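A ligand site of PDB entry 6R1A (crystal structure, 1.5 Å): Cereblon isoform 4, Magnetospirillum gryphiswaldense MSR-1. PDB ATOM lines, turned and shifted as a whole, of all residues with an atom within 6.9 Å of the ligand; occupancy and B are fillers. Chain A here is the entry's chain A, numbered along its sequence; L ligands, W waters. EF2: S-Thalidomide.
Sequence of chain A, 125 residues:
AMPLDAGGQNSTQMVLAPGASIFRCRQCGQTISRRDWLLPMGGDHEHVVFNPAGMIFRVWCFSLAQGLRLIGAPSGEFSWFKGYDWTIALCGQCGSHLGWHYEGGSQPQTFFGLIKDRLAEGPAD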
ATOM      1  N   VAL A  49     -13.387  20.248   2.088  1.00  0.00           N
ATOM      2  CA  VAL A  49     -14.460  19.641   2.854  1.00  0.00           C
ATOM      3  C   VAL A  49     -15.068  20.639   3.814  1.00  0.00           C
ATOM      4  O   VAL A  49     -14.461  21.679   4.078  1.00  0.00           O
ATOM      5  CB  VAL A  49     -13.923  18.426   3.649  1.00  0.00           C
ATOM      6  CG1 VAL A  49     -13.459  17.313   2.694  1.00  0.00           C
ATOM      7  CG2 VAL A  49     -12.781  18.821   4.589  1.00  0.00           C
ATOM      8  N   PHE A  50     -16.268  20.371   4.325  1.00  0.00           N
ATOM      9  CA  PHE A  50     -16.806  21.184   5.395  1.00  0.00           C
ATOM     10  C   PHE A  50     -17.379  20.377   6.527  1.00  0.00           C
ATOM     11  O   PHE A  50     -17.887  19.260   6.300  1.00  0.00           O
ATOM     12  CB  PHE A  50     -17.813  22.247   4.868  1.00  0.00           C
ATOM     13  CG  PHE A  50     -19.077  21.702   4.377  1.00  0.00           C
ATOM     14  CD1 PHE A  50     -19.265  21.387   3.032  1.00  0.00           C
ATOM     15  CD2 PHE A  50     -20.169  21.549   5.258  1.00  0.00           C
ATOM     16  CE1 PHE A  50     -20.494  20.899   2.588  1.00  0.00           C
ATOM     17  CE2 PHE A  50     -21.382  21.035   4.819  1.00  0.00           C
ATOM     18  CZ  PHE A  50     -21.549  20.729   3.491  1.00  0.00           C
ATOM     19  N   ASN A  51     -17.276  20.897   7.735  1.00  0.00           N
ATOM     20  CA  ASN A  51     -17.794  20.215   8.921  1.00  0.00           C
ATOM     21  C   ASN A  51     -19.258  20.641   9.231  1.00  0.00           C
ATOM     22  O   ASN A  51     -19.842  21.489   8.553  1.00  0.00           O
ATOM     23  CB  ASN A  51     -16.833  20.379  10.115  1.00  0.00           C
ATOM     24  CG  ASN A  51     -16.790  21.785  10.688  1.00  0.00           C
ATOM     25  OD1 ASN A  51     -17.609  22.646  10.347  1.00  0.00           O
ATOM     26  ND2 ASN A  51     -15.887  22.005  11.621  1.00  0.00           N
ATOM     27  N   PRO A  52     -19.866  20.049  10.276  1.00  0.00           N
ATOM     28  CA  PRO A  52     -21.268  20.406  10.580  1.00  0.00           C
ATOM     29  C   PRO A  52     -21.463  21.862  11.033  1.00  0.00           C
ATOM     30  O   PRO A  52     -22.592  22.372  10.958  1.00  0.00           O
ATOM     31  CB  PRO A  52     -21.655  19.438  11.706  1.00  0.00           C
ATOM     32  CG  PRO A  52     -20.745  18.265  11.502  1.00  0.00           C
ATOM     33  CD  PRO A  52     -19.428  18.883  11.074  1.00  0.00           C
ATOM     34  N   ALA A  53     -20.403  22.521  11.480  1.00  0.00           N
ATOM     35  CA  ALA A  53     -20.437  23.917  11.854  1.00  0.00           C
ATOM     36  C   ALA A  53     -20.220  24.828  10.650  1.00  0.00           C
ATOM     37  O   ALA A  53     -20.053  26.032  10.820  1.00  0.00           O
ATOM     38  CB  ALA A  53     -19.421  24.210  12.930  1.00  0.00           C
ATOM     39  N   MET A  55     -17.569  25.052   8.692  1.00  0.00           N
ATOM     40  CA  MET A  55     -16.195  25.474   8.459  1.00  0.00           C
ATOM     41  C   MET A  55     -15.653  24.681   7.285  1.00  0.00           C
ATOM     42  O   MET A  55     -15.780  23.453   7.250  1.00  0.00           O
ATOM     43  CB  MET A  55     -15.347  25.222   9.700  1.00  0.00           C
ATOM     44  CG  MET A  55     -13.925  25.661   9.528  1.00  0.00           C
ATOM     45  SD  MET A  55     -13.296  26.275  11.089  1.00  0.00           S
ATOM     46  CE  MET A  55     -14.371  27.699  11.246  1.00  0.00           C
ATOM     47  N   PHE A  57     -12.432  23.370   5.069  1.00  0.00           N
ATOM     48  CA  PHE A  57     -11.024  23.027   5.276  1.00  0.00           C
ATOM     49  C   PHE A  57     -10.480  22.510   3.961  1.00  0.00           C
ATOM     50  O   PHE A  57     -11.145  21.751   3.261  1.00  0.00           O
ATOM     51  CB  PHE A  57     -10.811  21.950   6.330  1.00  0.00           C
ATOM     52  CG  PHE A  57     -11.401  22.238   7.686  1.00  0.00           C
ATOM     53  CD1 PHE A  57     -10.685  22.928   8.638  1.00  0.00           C
ATOM     54  CD2 PHE A  57     -12.654  21.762   8.025  1.00  0.00           C
ATOM     55  CE1 PHE A  57     -11.228  23.201   9.891  1.00  0.00           C
ATOM     56  CE2 PHE A  57     -13.194  22.013   9.287  1.00  0.00           C
ATOM     57  CZ  PHE A  57     -12.462  22.713  10.225  1.00  0.00           C
ATOM     58  N   SER A  75     -14.207   8.162  15.865  1.00  0.00           N
ATOM     59  CA  SER A  75     -15.609   8.266  15.514  1.00  0.00           C
ATOM     60  C   SER A  75     -15.797   8.184  14.015  1.00  0.00           C
ATOM     61  O   SER A  75     -14.997   8.743  13.265  1.00  0.00           O
ATOM     62  CB  SER A  75     -16.154   9.621  15.975  1.00  0.00           C
ATOM     63  OG  SER A  75     -17.517   9.780  15.566  1.00  0.00           O
ATOM     64  N   GLY A  76     -16.830   7.495  13.561  1.00  0.00           N
ATOM     65  CA  GLY A  76     -17.194   7.485  12.154  1.00  0.00           C
ATOM     66  C   GLY A  76     -18.135   8.591  11.737  1.00  0.00           C
ATOM     67  O   GLY A  76     -18.383   8.758  10.559  1.00  0.00           O
ATOM     68  N   GLU A  77     -18.641   9.370  12.687  1.00  0.00           N
ATOM     69  CA  GLU A  77     -19.708  10.336  12.352  1.00  0.00           C
ATOM     70  C   GLU A  77     -19.161  11.469  11.466  1.00  0.00           C
ATOM     71  O   GLU A  77     -18.112  12.040  11.707  1.00  0.00           O
ATOM     72  CB  GLU A  77     -20.641  10.723  13.499  1.00  0.00           C
ATOM     73  CG  GLU A  77     -20.085  11.177  14.802  1.00  0.00           C
ATOM     74  CD  GLU A  77     -21.033  10.894  15.985  1.00  0.00           C
ATOM     75  OE1 GLU A  77     -21.708   9.841  16.001  1.00  0.00           O
ATOM     76  OE2 GLU A  77     -21.072  11.727  16.909  1.00  0.00           O
ATOM     77  N   PHE A  78     -19.898  11.730  10.406  1.00  0.00           N
ATOM     78  CA  PHE A  78     -19.589  12.803   9.435  1.00  0.00           C
ATOM     79  C   PHE A  78     -18.231  12.598   8.747  1.00  0.00           C
ATOM     80  O   PHE A  78     -17.698  13.550   8.224  1.00  0.00           O
ATOM     81  CB  PHE A  78     -19.602  14.226  10.072  1.00  0.00           C
ATOM     82  CG  PHE A  78     -20.787  14.509  10.930  1.00  0.00           C
ATOM     83  CD1 PHE A  78     -22.001  14.647  10.376  1.00  0.00           C
ATOM     84  CD2 PHE A  78     -20.668  14.609  12.301  1.00  0.00           C
ATOM     85  CE1 PHE A  78     -23.141  14.946  11.144  1.00  0.00           C
ATOM     86  CE2 PHE A  78     -21.771  14.876  13.110  1.00  0.00           C
ATOM     87  CZ  PHE A  78     -22.995  15.060  12.519  1.00  0.00           C
ATOM     88  N   SER A  79     -17.663  11.391   8.738  1.00  0.00           N
ATOM     89  CA  SER A  79     -16.361  11.211   8.136  1.00  0.00           C
ATOM     90  C   SER A  79     -16.366  11.593   6.669  1.00  0.00           C
ATOM     91  O   SER A  79     -17.214  11.170   5.900  1.00  0.00           O
ATOM     92  CB  SER A  79     -15.848   9.779   8.261  1.00  0.00           C
ATOM     93  OG  SER A  79     -14.560   9.699   7.707  1.00  0.00           O
ATOM     94  N   TRP A  80     -15.393  12.395   6.282  1.00  0.00           N
ATOM     95  CA  TRP A  80     -15.205  12.812   4.898  1.00  0.00           C
ATOM     96  C   TRP A  80     -14.606  11.701   4.037  1.00  0.00           C
ATOM     97  O   TRP A  80     -14.558  11.844   2.805  1.00  0.00           O
ATOM     98  CB  TRP A  80     -14.309  14.038   4.842  1.00  0.00           C
ATOM     99  CG  TRP A  80     -14.872  15.233   5.525  1.00  0.00           C
ATOM    100  CD1 TRP A  80     -16.126  15.791   5.366  1.00  0.00           C
ATOM    101  CD2 TRP A  80     -14.173  16.081   6.436  1.00  0.00           C
ATOM    102  NE1 TRP A  80     -16.243  16.915   6.146  1.00  0.00           N
ATOM    103  CE2 TRP A  80     -15.031  17.132   6.787  1.00  0.00           C
ATOM    104  CE3 TRP A  80     -12.885  16.055   6.979  1.00  0.00           C
ATOM    105  CZ2 TRP A  80     -14.656  18.114   7.691  1.00  0.00           C
ATOM    106  CZ3 TRP A  80     -12.525  17.034   7.855  1.00  0.00           C
ATOM    107  CH2 TRP A  80     -13.400  18.067   8.189  1.00  0.00           C
ATOM    108  N   PHE A  81     -14.132  10.610   4.636  1.00  0.00           N
ATOM    109  CA  PHE A  81     -13.452   9.543   3.913  1.00  0.00           C
ATOM    110  C   PHE A  81     -14.155   8.254   4.233  1.00  0.00           C
ATOM    111  O   PHE A  81     -14.135   7.775   5.354  1.00  0.00           O
ATOM    112  CB  PHE A  81     -11.961   9.518   4.290  1.00  0.00           C
ATOM    113  CG  PHE A  81     -11.250  10.790   3.958  1.00  0.00           C
ATOM    114  CD1 PHE A  81     -10.792  11.017   2.673  1.00  0.00           C
ATOM    115  CD2 PHE A  81     -11.040  11.731   4.916  1.00  0.00           C
ATOM    116  CE1 PHE A  81     -10.038  12.160   2.356  1.00  0.00           C
ATOM    117  CE2 PHE A  81     -10.376  12.929   4.601  1.00  0.00           C
ATOM    118  CZ  PHE A  81      -9.869  13.134   3.324  1.00  0.00           C
ATOM    119  N   TYR A  84     -13.519   5.245   7.007  1.00  0.00           N
ATOM    120  CA  TYR A  84     -12.553   5.647   8.026  1.00  0.00           C
ATOM    121  C   TYR A  84     -13.242   6.348   9.196  1.00  0.00           C
ATOM    122  O   TYR A  84     -14.211   7.069   9.003  1.00  0.00           O
ATOM    123  CB  TYR A  84     -11.533   6.609   7.451  1.00  0.00           C
ATOM    124  CG  TYR A  84     -10.662   6.021   6.411  1.00  0.00           C
ATOM    125  CD1 TYR A  84      -9.489   5.356   6.746  1.00  0.00           C
ATOM    126  CD2 TYR A  84     -10.978   6.131   5.071  1.00  0.00           C
ATOM    127  CE1 TYR A  84      -8.659   4.838   5.769  1.00  0.00           C
ATOM    128  CE2 TYR A  84     -10.167   5.582   4.086  1.00  0.00           C
ATOM    129  CZ  TYR A  84      -9.026   4.919   4.439  1.00  0.00           C
ATOM    130  OH  TYR A  84      -8.243   4.399   3.461  1.00  0.00           O
ATOM    131  N   TRP A  86     -12.338   8.816  12.568  1.00  0.00           N
ATOM    132  CA  TRP A  86     -11.375   9.917  12.799  1.00  0.00           C
ATOM    133  C   TRP A  86     -11.186  10.189  14.265  1.00  0.00           C
ATOM    134  O   TRP A  86     -12.086   9.954  15.101  1.00  0.00           O
ATOM    135  CB  TRP A  86     -11.807  11.208  12.108  1.00  0.00           C
ATOM    136  CG  TRP A  86     -13.215  11.640  12.426  1.00  0.00           C
ATOM    137  CD1 TRP A  86     -14.336  11.360  11.701  1.00  0.00           C
ATOM    138  CD2 TRP A  86     -13.641  12.400  13.553  1.00  0.00           C
ATOM    139  NE1 TRP A  86     -15.427  11.871  12.324  1.00  0.00           N
ATOM    140  CE2 TRP A  86     -15.039  12.523  13.467  1.00  0.00           C
ATOM    141  CE3 TRP A  86     -12.986  12.992  14.626  1.00  0.00           C
ATOM    142  CZ2 TRP A  86     -15.794  13.188  14.424  1.00  0.00           C
ATOM    143  CZ3 TRP A  86     -13.731  13.698  15.572  1.00  0.00           C
ATOM    144  CH2 TRP A  86     -15.119  13.810  15.443  1.00  0.00           C
ATOM    145  N   THR A  87     -10.004  10.747  14.548  1.00  0.00           N
ATOM    146  CA  THR A  87      -9.661  11.289  15.860  1.00  0.00           C
ATOM    147  C   THR A  87      -9.081  12.687  15.592  1.00  0.00           C
ATOM    148  O   THR A  87      -8.325  12.851  14.639  1.00  0.00           O
ATOM    149  CB  THR A  87      -8.580  10.360  16.449  1.00  0.00           C
ATOM    150  OG1 THR A  87      -9.108   9.018  16.545  1.00  0.00           O
ATOM    151  CG2 THR A  87      -8.133  10.734  17.731  1.00  0.00           C
ATOM    152  N   ILE A  88      -9.403  13.627  16.458  1.00  0.00           N
ATOM    153  CA  ILE A  88      -8.800  14.977  16.347  1.00  0.00           C
ATOM    154  C   ILE A  88      -7.298  14.865  16.585  1.00  0.00           C
ATOM    155  O   ILE A  88      -6.830  14.133  17.507  1.00  0.00           O
ATOM    156  CB  ILE A  88      -9.467  15.898  17.378  1.00  0.00           C
ATOM    157  CG1 ILE A  88     -10.912  16.145  16.929  1.00  0.00           C
ATOM    158  CG2 ILE A  88      -8.668  17.213  17.582  1.00  0.00           C
ATOM    159  CD1 ILE A  88     -11.789  16.721  18.021  1.00  0.00           C
ATOM    160  N   HIS A  97      -5.173  22.928  16.591  1.00  0.00           N
ATOM    161  CA  HIS A  97      -5.853  21.836  15.901  1.00  0.00           C
ATOM    162  C   HIS A  97      -5.363  21.758  14.473  1.00  0.00           C
ATOM    163  O   HIS A  97      -5.675  22.639  13.657  1.00  0.00           O
ATOM    164  CB  HIS A  97      -7.361  22.050  15.946  1.00  0.00           C
ATOM    165  CG  HIS A  97      -8.107  21.026  15.180  1.00  0.00           C
ATOM    166  ND1 HIS A  97      -9.323  21.273  14.580  1.00  0.00           N
ATOM    167  CD2 HIS A  97      -7.801  19.733  14.885  1.00  0.00           C
ATOM    168  CE1 HIS A  97      -9.729  20.180  13.975  1.00  0.00           C
ATOM    169  NE2 HIS A  97      -8.825  19.234  14.130  1.00  0.00           N
ATOM    170  N   TRP A 100      -6.827  15.666  11.535  1.00  0.00           N
ATOM    171  CA  TRP A 100      -7.411  14.435  12.046  1.00  0.00           C
ATOM    172  C   TRP A 100      -6.586  13.252  11.615  1.00  0.00           C
ATOM    173  O   TRP A 100      -5.938  13.268  10.567  1.00  0.00           O
ATOM    174  CB  TRP A 100      -8.851  14.238  11.506  1.00  0.00           C
ATOM    175  CG  TRP A 100      -9.762  15.420  11.792  1.00  0.00           C
ATOM    176  CD1 TRP A 100     -10.587  15.556  12.864  1.00  0.00           C
ATOM    177  CD2 TRP A 100      -9.877  16.629  11.039  1.00  0.00           C
ATOM    178  NE1 TRP A 100     -11.217  16.787  12.805  1.00  0.00           N
ATOM    179  CE2 TRP A 100     -10.795  17.460  11.701  1.00  0.00           C
ATOM    180  CE3 TRP A 100      -9.291  17.093   9.860  1.00  0.00           C
ATOM    181  CZ2 TRP A 100     -11.137  18.729  11.235  1.00  0.00           C
ATOM    182  CZ3 TRP A 100      -9.634  18.385   9.395  1.00  0.00           C
ATOM    183  CH2 TRP A 100     -10.523  19.178  10.100  1.00  0.00           C
ATOM    184  N   TYR A 102      -7.065   9.325  10.617  1.00  0.00           N
ATOM    185  CA  TYR A 102      -8.101   8.423  10.113  1.00  0.00           C
ATOM    186  C   TYR A 102      -7.617   6.984  10.255  1.00  0.00           C
ATOM    187  O   TYR A 102      -6.463   6.697  10.027  1.00  0.00           O
ATOM    188  CB  TYR A 102      -8.405   8.733   8.646  1.00  0.00           C
ATOM    189  CG  TYR A 102      -9.148  10.038   8.523  1.00  0.00           C
ATOM    190  CD1 TYR A 102     -10.518  10.075   8.632  1.00  0.00           C
ATOM    191  CD2 TYR A 102      -8.455  11.238   8.365  1.00  0.00           C
ATOM    192  CE1 TYR A 102     -11.220  11.273   8.526  1.00  0.00           C
ATOM    193  CE2 TYR A 102      -9.122  12.434   8.252  1.00  0.00           C
ATOM    194  CZ  TYR A 102     -10.502  12.452   8.373  1.00  0.00           C
ATOM    195  OH  TYR A 102     -11.221  13.640   8.270  1.00  0.00           O
HETATM  196  O01 EF2 L   1     -17.102  16.719   9.749  1.00  0.00           O
HETATM  197  C02 EF2 L   1     -16.027  16.228  10.030  1.00  0.00           C
HETATM  198  N03 EF2 L   1     -15.503  15.182   9.290  1.00  0.00           N
HETATM  199  C04 EF2 L   1     -14.330  14.508   9.533  1.00  0.00           C
HETATM  200  O05 EF2 L   1     -13.951  13.642   8.760  1.00  0.00           O
HETATM  201  C06 EF2 L   1     -13.553  14.878  10.755  1.00  0.00           C
HETATM  202  C07 EF2 L   1     -14.391  15.560  11.822  1.00  0.00           C
HETATM  203  C08 EF2 L   1     -15.171  16.706  11.199  1.00  0.00           C
HETATM  204  N09 EF2 L   1     -15.974  17.422  12.179  1.00  0.00           N
HETATM  205  C11 EF2 L   1     -17.798  20.050  15.485  1.00  0.00           C
HETATM  206  C12 EF2 L   1     -16.765  20.072  14.570  1.00  0.00           C
HETATM  207  C13 EF2 L   1     -16.604  18.951  13.781  1.00  0.00           C
HETATM  208  C14 EF2 L   1     -17.434  17.854  13.900  1.00  0.00           C
HETATM  209  O16 EF2 L   1     -14.658  19.313  12.358  1.00  0.00           O
HETATM  210  O18 EF2 L   1     -17.394  15.697  12.765  1.00  0.00           O
HETATM  211  C19 EF2 L   1     -18.462  17.824  14.814  1.00  0.00           C
HETATM  212  C20 EF2 L   1     -18.634  18.949  15.615  1.00  0.00           C
HETATM  213  C3  EF2 L   1     -16.989  16.827  12.922  1.00  0.00           C
HETATM  214  C4  EF2 L   1     -15.604  18.656  12.716  1.00  0.00           C
HETATM  215  O   HOH W   1     -13.123  18.004  14.502  1.00  0.00           O
HETATM  216  O   HOH W   2     -18.675  14.572  15.691  1.00  0.00           O
HETATM  217  O   HOH W   3     -12.985  20.550  13.672  1.00  0.00           O
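OH of Tyr 102 is in hydrogen-bond range of O05 of the ligand (2.8 Å).
A nitrogen (N03) of the ligand is in hydrogen-bond range of the backbone carbonyl oxygen of Phe 78 (2.9 Å).
The side-chain amide nitrogen (ND2) of Asn 51 is in hydrogen-bond range of an oxygen (O16) of the ligand (3.0 Å).
The backbone NH (N) of Trp 80 sits at hydrogen-bond distance from an oxygen (O05) of the ligand, 3.1 Å away.
The side-chain amide oxygen of Asn 51 lies within hydrogen-bond range of the backbone NH of Ala 53 (3.0 Å).
The side-chain amide oxygen of Asn 51 is in hydrogen-bond range of the backbone NH of Met 55.
The backbone carbonyl oxygen (O) of Phe 50 sits at hydrogen-bond distance from the indole nitrogen (NE1) of Trp 80, 2.9 Å away.
NE1 of Trp 86 is in hydrogen-bond range of O of Glu 77 (2.8 Å).
O of Ser 75 lies within hydrogen-bond range of N of Trp 86 (2.7 Å).
OG of Ser 79 lies within hydrogen-bond range of O of Phe 81, at 3.1 Å.
The side-chain hydroxyl of Ser 79 lies within hydrogen-bond range of the backbone carbonyl oxygen of Tyr 84 (3.0 Å).
The backbone NH of Glu 77 sits close to the side-chain hydroxyl of Ser 75.
Residues that only touch the ligand: Pro 52 (3.4 Å), Glu 77 (3.9 Å), Ser 79 (3.5 Å), Trp 86 (3.4 Å) and Trp 100 (3.5 Å).
Hydrophobic or aromatic side chains within 4 Å of the ligand: Pro 52, Phe 78, Trp 80, Trp 86, Trp 100 and Tyr 102.
Of the 21 residues printed, 9 come within 4 Å of the ligand.
The nearest printed residue that does not touch the ligand is Phe 57 (4.3 Å).
Water W1 lies within hydrogen-bond range of the indole nitrogen of Trp 100 (2.8 Å) and an oxygen (O16) of the ligand (2.9 Å).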
